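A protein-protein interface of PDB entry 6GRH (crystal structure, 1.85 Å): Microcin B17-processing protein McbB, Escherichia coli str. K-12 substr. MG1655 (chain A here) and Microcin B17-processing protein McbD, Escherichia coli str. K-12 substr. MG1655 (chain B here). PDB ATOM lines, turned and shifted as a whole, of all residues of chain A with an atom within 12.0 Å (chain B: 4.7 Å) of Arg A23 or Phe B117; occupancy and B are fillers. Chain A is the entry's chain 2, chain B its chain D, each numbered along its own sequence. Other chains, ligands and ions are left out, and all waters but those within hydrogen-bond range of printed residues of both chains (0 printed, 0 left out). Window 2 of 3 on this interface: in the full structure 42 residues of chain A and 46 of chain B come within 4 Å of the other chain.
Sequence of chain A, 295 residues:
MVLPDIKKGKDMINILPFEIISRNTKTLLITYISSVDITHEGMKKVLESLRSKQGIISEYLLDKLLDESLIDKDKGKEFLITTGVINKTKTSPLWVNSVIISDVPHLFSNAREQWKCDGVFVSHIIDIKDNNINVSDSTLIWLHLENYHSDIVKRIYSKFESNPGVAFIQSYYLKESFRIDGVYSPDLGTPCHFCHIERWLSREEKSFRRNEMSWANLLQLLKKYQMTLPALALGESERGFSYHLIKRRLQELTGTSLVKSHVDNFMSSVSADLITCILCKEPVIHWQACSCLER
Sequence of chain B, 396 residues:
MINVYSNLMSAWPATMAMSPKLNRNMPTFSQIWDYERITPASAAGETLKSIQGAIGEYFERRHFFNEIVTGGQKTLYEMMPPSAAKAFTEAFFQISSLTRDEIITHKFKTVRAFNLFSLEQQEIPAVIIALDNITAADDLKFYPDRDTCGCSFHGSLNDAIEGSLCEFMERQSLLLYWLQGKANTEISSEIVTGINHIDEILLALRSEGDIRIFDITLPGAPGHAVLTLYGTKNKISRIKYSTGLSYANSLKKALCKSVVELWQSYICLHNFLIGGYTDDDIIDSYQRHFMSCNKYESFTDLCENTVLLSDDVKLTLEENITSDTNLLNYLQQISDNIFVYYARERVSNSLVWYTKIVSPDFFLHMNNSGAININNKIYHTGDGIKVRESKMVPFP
NH2 of Arg A23 is in hydrogen-bond range of O of Leu B116, 2.9 Å away.
OD1 of Asn B115 is in hydrogen-bond range of N of Phe B117, at 2.9 Å. The backbone NH (N) of Leu B116 sits at hydrogen-bond distance from the backbone carbonyl oxygen (O) of Ile B338, 2.8 Å away. The backbone NH (N) of Ile A21 lies within hydrogen-bond range of the backbone carbonyl oxygen (O) of Leu A28. OD1 of Asn B115 is in hydrogen-bond range of N of Ser B118 (3.0 Å).
Ile A21 touches Leu B119 (O to CD1, 3.3 Å). Arg A23 touches Phe B117. Arg A23 touches Leu B119. Leu B328 touches Arg A23 (CD1 to CZ, 3.4 Å). CG of Lys A26 touches O of Ser B118, at 3.6 Å. O of Lys A26 touches CD1 of Leu B119, 3.8 Å away.
Glu A19 touches none of the printed residues of chain B. Of the printed residues of chain B, Ile A21 touches Leu B119. Ser A22 touches none of the printed residues of chain B. Printed residues of chain B within 4 Å of Arg A23: Leu B116, Phe B117, Leu B119 and Leu B328. Of the printed residues of chain B, Lys A26 touches Ser B118 (3.6 Å) and Leu B119 (3.8 Å). Phe B117 touches just one residue of chain A: Arg A23. Ser B118 touches one residue of chain A. Printed residues of chain A within 4 Å of Leu B119: Ile A21 (3.3 Å), Arg A23 (3.99 Å) and Lys A26 (3.8 Å). No residue of chain A comes within 4 Å of Leu B331. No residue of chain A comes within 4 Å of Ser B335. No residue of chain A comes within 4 Å of Ile B338. The nearest printed residue of chain B that does not touch Arg A23 is Ser B118 (5.4 Å).
Printed residues of chain B that touch a printed residue of chain A: Leu B116, Phe B117, Ser B118, Leu B119 and Leu B328. Printed residues of chain A that touch a printed residue of chain B: Ile A21, Arg A23 and Lys A26. Among the printed residues, 7 pairs touch across the chains. Among the printed residues, no Asp or Glu carboxylate lies within 4 Å of a Lys or Arg side-chain nitrogen of the other chain.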
ATOM      1  N   GLU A  19      -2.139   1.152  15.873  1.00  0.00           N
ATOM      2  CA  GLU A  19      -1.726  -0.084  16.530  1.00  0.00           C
ATOM      3  C   GLU A  19      -0.331   0.068  17.130  1.00  0.00           C
ATOM      4  O   GLU A  19       0.502   0.795  16.586  1.00  0.00           O
ATOM      5  CB  GLU A  19      -1.707  -1.225  15.512  1.00  0.00           C
ATOM      6  CG  GLU A  19      -3.071  -1.669  15.005  1.00  0.00           C
ATOM      7  CD  GLU A  19      -3.882  -2.510  15.976  1.00  0.00           C
ATOM      8  OE1 GLU A  19      -3.424  -2.811  17.098  1.00  0.00           O
ATOM      9  OE2 GLU A  19      -4.998  -2.912  15.592  1.00  0.00           O
ATOM     10  N   ILE A  20      -0.107  -0.627  18.251  1.00  0.00           N
ATOM     11  CA  ILE A  20       1.230  -0.867  18.783  1.00  0.00           C
ATOM     12  C   ILE A  20       1.408  -2.365  18.866  1.00  0.00           C
ATOM     13  O   ILE A  20       0.532  -3.068  19.359  1.00  0.00           O
ATOM     14  CB  ILE A  20       1.518  -0.260  20.195  1.00  0.00           C
ATOM     15  CG1 ILE A  20       0.285  -0.258  21.090  1.00  0.00           C
ATOM     16  CG2 ILE A  20       2.039   1.162  20.067  1.00  0.00           C
ATOM     17  CD1 ILE A  20       0.614  -0.108  22.572  1.00  0.00           C
ATOM     18  N   ILE A  21       2.539  -2.855  18.392  1.00  0.00           N
ATOM     19  CA  ILE A  21       2.870  -4.281  18.535  1.00  0.00           C
ATOM     20  C   ILE A  21       4.154  -4.350  19.358  1.00  0.00           C
ATOM     21  O   ILE A  21       5.082  -3.570  19.116  1.00  0.00           O
ATOM     22  CB  ILE A  21       2.956  -5.012  17.157  1.00  0.00           C
ATOM     23  CG1 ILE A  21       3.473  -6.449  17.325  1.00  0.00           C
ATOM     24  CG2 ILE A  21       3.833  -4.260  16.161  1.00  0.00           C
ATOM     25  CD1 ILE A  21       3.388  -7.278  16.050  1.00  0.00           C
ATOM     26  N   SER A  22       4.183  -5.247  20.346  1.00  0.00           N
ATOM     27  CA  SER A  22       5.343  -5.402  21.217  1.00  0.00           C
ATOM     28  C   SER A  22       5.916  -6.813  21.191  1.00  0.00           C
ATOM     29  O   SER A  22       5.185  -7.792  21.065  1.00  0.00           O
ATOM     30  CB  SER A  22       5.001  -4.989  22.651  1.00  0.00           C
ATOM     31  OG  SER A  22       4.904  -3.576  22.708  1.00  0.00           O
ATOM     32  N   ARG A  23       7.238  -6.892  21.279  1.00  0.00           N
ATOM     33  CA  ARG A  23       7.960  -8.166  21.336  1.00  0.00           C
ATOM     34  C   ARG A  23       9.125  -7.989  22.292  1.00  0.00           C
ATOM     35  O   ARG A  23      10.109  -7.299  21.969  1.00  0.00           O
ATOM     36  CB  ARG A  23       8.431  -8.598  19.932  1.00  0.00           C
ATOM     37  CG  ARG A  23       8.378 -10.107  19.733  1.00  0.00           C
ATOM     38  CD  ARG A  23       6.960 -10.572  19.479  1.00  0.00           C
ATOM     39  NE  ARG A  23       6.609 -10.535  18.062  1.00  0.00           N
ATOM     40  CZ  ARG A  23       5.367 -10.527  17.567  1.00  0.00           C
ATOM     41  NH1 ARG A  23       4.295 -10.516  18.359  1.00  0.00           N
ATOM     42  NH2 ARG A  23       5.194 -10.517  16.251  1.00  0.00           N
ATOM     43  N   ASN A  24       8.988  -8.584  23.481  1.00  0.00           N
ATOM     44  CA  ASN A  24       9.851  -8.285  24.613  1.00  0.00           C
ATOM     45  C   ASN A  24       9.871  -6.752  24.826  1.00  0.00           C
ATOM     46  O   ASN A  24       8.810  -6.155  25.068  1.00  0.00           O
ATOM     47  CB  ASN A  24      11.248  -8.889  24.401  1.00  0.00           C
ATOM     48  N   THR A  25      11.043  -6.128  24.669  1.00  0.00           N
ATOM     49  CA  THR A  25      11.226  -4.684  24.860  1.00  0.00           C
ATOM     50  C   THR A  25      11.151  -3.893  23.547  1.00  0.00           C
ATOM     51  O   THR A  25      11.383  -2.686  23.539  1.00  0.00           O
ATOM     52  CB  THR A  25      12.603  -4.412  25.497  1.00  0.00           C
ATOM     53  OG1 THR A  25      13.621  -4.792  24.561  1.00  0.00           O
ATOM     54  CG2 THR A  25      12.773  -5.206  26.819  1.00  0.00           C
ATOM     55  N   LYS A  26      10.842  -4.570  22.442  1.00  0.00           N
ATOM     56  CA  LYS A  26      10.695  -3.907  21.153  1.00  0.00           C
ATOM     57  C   LYS A  26       9.233  -3.497  21.006  1.00  0.00           C
ATOM     58  O   LYS A  26       8.341  -4.299  21.291  1.00  0.00           O
ATOM     59  CB  LYS A  26      11.074  -4.862  20.018  1.00  0.00           C
ATOM     60  CG  LYS A  26      12.456  -5.503  20.140  1.00  0.00           C
ATOM     61  CD  LYS A  26      13.596  -4.487  20.201  1.00  0.00           C
ATOM     62  CE  LYS A  26      13.697  -3.631  18.938  1.00  0.00           C
ATOM     63  NZ  LYS A  26      14.545  -2.447  19.228  1.00  0.00           N
ATOM     64  N   THR A  27       8.993  -2.269  20.548  1.00  0.00           N
ATOM     65  CA  THR A  27       7.635  -1.768  20.338  1.00  0.00           C
ATOM     66  C   THR A  27       7.616  -1.050  19.003  1.00  0.00           C
ATOM     67  O   THR A  27       8.493  -0.245  18.734  1.00  0.00           O
ATOM     68  CB  THR A  27       7.162  -0.834  21.480  1.00  0.00           C
ATOM     69  OG1 THR A  27       7.082  -1.570  22.709  1.00  0.00           O
ATOM     70  CG2 THR A  27       5.794  -0.280  21.206  1.00  0.00           C
ATOM     71  N   LEU A  28       6.623  -1.376  18.179  1.00  0.00           N
ATOM     72  CA  LEU A  28       6.426  -0.730  16.888  1.00  0.00           C
ATOM     73  C   LEU A  28       5.014  -0.123  16.849  1.00  0.00           C
ATOM     74  O   LEU A  28       4.026  -0.805  17.163  1.00  0.00           O
ATOM     75  CB  LEU A  28       6.628  -1.765  15.772  1.00  0.00           C
ATOM     76  CG  LEU A  28       6.272  -1.383  14.327  1.00  0.00           C
ATOM     77  CD1 LEU A  28       7.164  -0.238  13.878  1.00  0.00           C
ATOM     78  CD2 LEU A  28       6.364  -2.571  13.370  1.00  0.00           C
ATOM     79  N   LEU A  29       4.949   1.154  16.470  1.00  0.00           N
ATOM     80  CA  LEU A  29       3.718   1.933  16.342  1.00  0.00           C
ATOM     81  C   LEU A  29       3.407   2.048  14.857  1.00  0.00           C
ATOM     82  O   LEU A  29       4.298   2.358  14.067  1.00  0.00           O
ATOM     83  CB  LEU A  29       3.913   3.350  16.921  1.00  0.00           C
ATOM     84  CG  LEU A  29       2.915   4.465  16.506  1.00  0.00           C
ATOM     85  CD1 LEU A  29       1.553   4.194  17.120  1.00  0.00           C
ATOM     86  CD2 LEU A  29       3.401   5.868  16.874  1.00  0.00           C
ATOM     87  N   ILE A  30       2.162   1.796  14.471  1.00  0.00           N
ATOM     88  CA  ILE A  30       1.741   2.009  13.097  1.00  0.00           C
ATOM     89  C   ILE A  30       0.426   2.772  13.094  1.00  0.00           C
ATOM     90  O   ILE A  30      -0.550   2.311  13.655  1.00  0.00           O
ATOM     91  CB  ILE A  30       1.608   0.690  12.304  1.00  0.00           C
ATOM     92  CG1 ILE A  30       2.887  -0.156  12.464  1.00  0.00           C
ATOM     93  CG2 ILE A  30       1.313   0.999  10.827  1.00  0.00           C
ATOM     94  CD1 ILE A  30       2.849  -1.485  11.736  1.00  0.00           C
ATOM     95  N   VAL A  36       6.702   3.578  13.341  1.00  0.00           N
ATOM     96  CA  VAL A  36       7.747   4.141  14.195  1.00  0.00           C
ATOM     97  C   VAL A  36       8.212   3.125  15.223  1.00  0.00           C
ATOM     98  O   VAL A  36       7.392   2.543  15.931  1.00  0.00           O
ATOM     99  CB  VAL A  36       7.255   5.394  14.977  1.00  0.00           C
ATOM    100  CG1 VAL A  36       8.416   6.093  15.664  1.00  0.00           C
ATOM    101  CG2 VAL A  36       6.535   6.369  14.054  1.00  0.00           C
ATOM    102  N   ASP A  37       9.529   2.951  15.319  1.00  0.00           N
ATOM    103  CA  ASP A  37      10.130   2.162  16.399  1.00  0.00           C
ATOM    104  C   ASP A  37       9.988   3.013  17.648  1.00  0.00           C
ATOM    105  O   ASP A  37      10.411   4.156  17.651  1.00  0.00           O
ATOM    106  CB  ASP A  37      11.629   1.894  16.159  1.00  0.00           C
ATOM    107  CG  ASP A  37      11.944   1.452  14.736  1.00  0.00           C
ATOM    108  OD1 ASP A  37      11.091   0.834  14.073  1.00  0.00           O
ATOM    109  OD2 ASP A  37      13.074   1.715  14.285  1.00  0.00           O
ATOM    110  N   ILE A  38       9.385   2.465  18.696  1.00  0.00           N
ATOM    111  CA  ILE A  38       9.197   3.203  19.932  1.00  0.00           C
ATOM    112  C   ILE A  38      10.188   2.615  20.913  1.00  0.00           C
ATOM    113  O   ILE A  38      10.014   1.482  21.369  1.00  0.00           O
ATOM    114  CB  ILE A  38       7.749   3.065  20.480  1.00  0.00           C
ATOM    115  CG1 ILE A  38       6.699   3.484  19.425  1.00  0.00           C
ATOM    116  CG2 ILE A  38       7.589   3.867  21.772  1.00  0.00           C
ATOM    117  CD1 ILE A  38       6.822   4.911  18.922  1.00  0.00           C
ATOM    118  N   THR A  39      11.225   3.387  21.237  1.00  0.00           N
ATOM    119  CA  THR A  39      12.272   2.954  22.153  1.00  0.00           C
ATOM    120  C   THR A  39      12.264   3.684  23.505  1.00  0.00           C
ATOM    121  O   THR A  39      13.037   3.303  24.379  1.00  0.00           O
ATOM    122  CB  THR A  39      13.667   3.126  21.508  1.00  0.00           C
ATOM    123  OG1 THR A  39      13.945   4.520  21.318  1.00  0.00           O
ATOM    124  CG2 THR A  39      13.745   2.406  20.159  1.00  0.00           C
ATOM    125  N   GLU A  41      10.416   4.389  27.059  1.00  0.00           N
ATOM    126  CA  GLU A  41       9.437   3.721  27.929  1.00  0.00           C
ATOM    127  C   GLU A  41       8.214   4.602  28.191  1.00  0.00           C
ATOM    128  O   GLU A  41       7.076   4.126  28.191  1.00  0.00           O
ATOM    129  CB  GLU A  41      10.070   3.351  29.276  1.00  0.00           C
ATOM    130  CG  GLU A  41       9.465   2.106  29.904  1.00  0.00           C
ATOM    131  CD  GLU A  41      10.155   0.834  29.439  1.00  0.00           C
ATOM    132  OE1 GLU A  41      11.154   0.449  30.080  1.00  0.00           O
ATOM    133  OE2 GLU A  41       9.699   0.221  28.448  1.00  0.00           O
ATOM    134  N   LYS A  44       5.894   4.655  25.139  1.00  0.00           N
ATOM    135  CA  LYS A  44       5.150   3.385  25.105  1.00  0.00           C
ATOM    136  C   LYS A  44       3.930   3.463  26.039  1.00  0.00           C
ATOM    137  O   LYS A  44       2.841   3.059  25.650  1.00  0.00           O
ATOM    138  CB  LYS A  44       6.049   2.195  25.495  1.00  0.00           C
ATOM    139  N   GLU A  48       0.131   3.194  24.908  1.00  0.00           N
ATOM    140  CA  GLU A  48      -0.740   2.157  25.513  1.00  0.00           C
ATOM    141  C   GLU A  48      -2.007   2.737  26.141  1.00  0.00           C
ATOM    142  O   GLU A  48      -3.079   2.135  26.032  1.00  0.00           O
ATOM    143  CB  GLU A  48       0.006   1.322  26.569  1.00  0.00           C
ATOM    144  CG  GLU A  48       0.782   0.173  25.948  1.00  0.00           C
ATOM    145  CD  GLU A  48       1.664  -0.585  26.928  1.00  0.00           C
ATOM    146  OE1 GLU A  48       1.381  -0.619  28.152  1.00  0.00           O
ATOM    147  OE2 GLU A  48       2.668  -1.164  26.461  1.00  0.00           O
ATOM    148  N   ASN B 115      10.307  -7.543  10.488  1.00  0.00           N
ATOM    149  CA  ASN B 115      10.703  -8.874  10.934  1.00  0.00           C
ATOM    150  C   ASN B 115       9.749  -9.328  12.044  1.00  0.00           C
ATOM    151  O   ASN B 115       9.529  -8.613  13.024  1.00  0.00           O
ATOM    152  CB  ASN B 115      12.171  -8.857  11.413  1.00  0.00           C
ATOM    153  CG  ASN B 115      12.665 -10.221  11.896  1.00  0.00           C
ATOM    154  OD1 ASN B 115      12.331 -10.675  12.997  1.00  0.00           O
ATOM    155  ND2 ASN B 115      13.487 -10.866  11.083  1.00  0.00           N
ATOM    156  N   LEU B 116       9.189 -10.523  11.883  1.00  0.00           N
ATOM    157  CA  LEU B 116       8.185 -11.060  12.806  1.00  0.00           C
ATOM    158  C   LEU B 116       8.640 -11.090  14.282  1.00  0.00           C
ATOM    159  O   LEU B 116       7.826 -10.902  15.188  1.00  0.00           O
ATOM    160  CB  LEU B 116       7.787 -12.476  12.368  1.00  0.00           C
ATOM    161  CG  LEU B 116       6.741 -13.241  13.188  1.00  0.00           C
ATOM    162  CD1 LEU B 116       5.415 -12.526  13.141  1.00  0.00           C
ATOM    163  CD2 LEU B 116       6.574 -14.670  12.667  1.00  0.00           C
ATOM    164  N   PHE B 117       9.928 -11.309  14.504  1.00  0.00           N
ATOM    165  CA  PHE B 117      10.466 -11.489  15.852  1.00  0.00           C
ATOM    166  C   PHE B 117      11.065 -10.214  16.453  1.00  0.00           C
ATOM    167  O   PHE B 117      10.822  -9.917  17.623  1.00  0.00           O
ATOM    168  CB  PHE B 117      11.505 -12.600  15.841  1.00  0.00           C
ATOM    169  CG  PHE B 117      11.058 -13.829  15.106  1.00  0.00           C
ATOM    170  CD1 PHE B 117      10.034 -14.607  15.614  1.00  0.00           C
ATOM    171  CD2 PHE B 117      11.649 -14.190  13.899  1.00  0.00           C
ATOM    172  CE1 PHE B 117       9.609 -15.740  14.935  1.00  0.00           C
ATOM    173  CE2 PHE B 117      11.233 -15.317  13.215  1.00  0.00           C
ATOM    174  CZ  PHE B 117      10.216 -16.100  13.737  1.00  0.00           C
ATOM    175  N   SER B 118      11.853  -9.473  15.680  1.00  0.00           N
ATOM    176  CA  SER B 118      12.535  -8.268  16.190  1.00  0.00           C
ATOM    177  C   SER B 118      11.737  -6.971  15.983  1.00  0.00           C
ATOM    178  O   SER B 118      12.084  -5.942  16.564  1.00  0.00           O
ATOM    179  CB  SER B 118      13.898  -8.119  15.509  1.00  0.00           C
ATOM    180  OG  SER B 118      13.739  -7.698  14.168  1.00  0.00           O
ATOM    181  N   LEU B 119      10.691  -7.026  15.150  1.00  0.00           N
ATOM    182  CA  LEU B 119       9.964  -5.847  14.667  1.00  0.00           C
ATOM    183  C   LEU B 119      10.826  -4.844  13.886  1.00  0.00           C
ATOM    184  O   LEU B 119      10.385  -3.719  13.652  1.00  0.00           O
ATOM    185  CB  LEU B 119       9.182  -5.145  15.800  1.00  0.00           C
ATOM    186  CG  LEU B 119       8.308  -6.074  16.652  1.00  0.00           C
ATOM    187  CD1 LEU B 119       7.516  -5.248  17.655  1.00  0.00           C
ATOM    188  CD2 LEU B 119       7.385  -6.920  15.777  1.00  0.00           C
ATOM    189  N   LEU B 328       5.916 -18.494  18.060  1.00  0.00           N
ATOM    190  CA  LEU B 328       6.991 -17.588  17.630  1.00  0.00           C
ATOM    191  C   LEU B 328       8.385 -18.116  17.986  1.00  0.00           C
ATOM    192  O   LEU B 328       9.311 -17.997  17.171  1.00  0.00           O
ATOM    193  CB  LEU B 328       6.799 -16.164  18.190  1.00  0.00           C
ATOM    194  CG  LEU B 328       5.642 -15.290  17.648  1.00  0.00           C
ATOM    195  CD1 LEU B 328       5.735 -13.868  18.194  1.00  0.00           C
ATOM    196  CD2 LEU B 328       5.600 -15.234  16.134  1.00  0.00           C
ATOM    197  N   LEU B 331       9.081 -21.065  15.568  1.00  0.00           N
ATOM    198  CA  LEU B 331       9.432 -20.586  14.223  1.00  0.00           C
ATOM    199  C   LEU B 331      10.820 -19.962  14.173  1.00  0.00           C
ATOM    200  O   LEU B 331      11.587 -20.235  13.244  1.00  0.00           O
ATOM    201  CB  LEU B 331       8.394 -19.587  13.697  1.00  0.00           C
ATOM    202  CG  LEU B 331       7.067 -20.238  13.298  1.00  0.00           C
ATOM    203  CD1 LEU B 331       5.990 -19.203  13.037  1.00  0.00           C
ATOM    204  CD2 LEU B 331       7.232 -21.185  12.119  1.00  0.00           C
ATOM    205  N   GLN B 332      11.145 -19.153  15.178  1.00  0.00           N
ATOM    206  CA  GLN B 332      12.439 -18.475  15.233  1.00  0.00           C
ATOM    207  C   GLN B 332      13.612 -19.444  15.328  1.00  0.00           C
ATOM    208  O   GLN B 332      14.678 -19.140  14.819  1.00  0.00           O
ATOM    209  CB  GLN B 332      12.509 -17.459  16.377  1.00  0.00           C
ATOM    210  CG  GLN B 332      13.692 -16.508  16.233  1.00  0.00           C
ATOM    211  CD  GLN B 332      13.676 -15.368  17.226  1.00  0.00           C
ATOM    212  OE1 GLN B 332      12.955 -15.404  18.230  1.00  0.00           O
ATOM    213  NE2 GLN B 332      14.482 -14.341  16.951  1.00  0.00           N
ATOM    214  N   SER B 335      14.165 -20.357  11.771  1.00  0.00           N
ATOM    215  CA  SER B 335      14.733 -19.227  11.016  1.00  0.00           C
ATOM    216  C   SER B 335      14.329 -17.872  11.574  1.00  0.00           C
ATOM    217  O   SER B 335      13.156 -17.657  11.844  1.00  0.00           O
ATOM    218  CB  SER B 335      14.265 -19.280   9.557  1.00  0.00           C
ATOM    219  OG  SER B 335      14.717 -18.140   8.830  1.00  0.00           O
ATOM    220  N   ASP B 336      15.291 -16.945  11.660  1.00  0.00           N
ATOM    221  CA  ASP B 336      15.017 -15.544  12.016  1.00  0.00           C
ATOM    222  C   ASP B 336      14.403 -14.746  10.855  1.00  0.00           C
ATOM    223  O   ASP B 336      13.924 -13.639  11.073  1.00  0.00           O
ATOM    224  CB  ASP B 336      16.301 -14.827  12.482  1.00  0.00           C
ATOM    225  CG  ASP B 336      16.912 -15.447  13.750  1.00  0.00           C
ATOM    226  OD1 ASP B 336      16.172 -16.108  14.500  1.00  0.00           O
ATOM    227  OD2 ASP B 336      18.138 -15.292  14.004  1.00  0.00           O
ATOM    228  N   ILE B 338      11.692 -14.338   8.912  1.00  0.00           N
ATOM    229  CA  ILE B 338      10.254 -14.379   8.684  1.00  0.00           C
ATOM    230  C   ILE B 338       9.773 -12.939   8.815  1.00  0.00           C
ATOM    231  O   ILE B 338      10.058 -12.264   9.818  1.00  0.00           O
ATOM    232  CB  ILE B 338       9.504 -15.289   9.677  1.00  0.00           C
ATOM    233  CG1 ILE B 338      10.128 -16.680   9.711  1.00  0.00           C
ATOM    234  CG2 ILE B 338       8.031 -15.399   9.289  1.00  0.00           C
ATOM    235  CD1 ILE B 338       9.410 -17.675  10.612  1.00  0.00           C
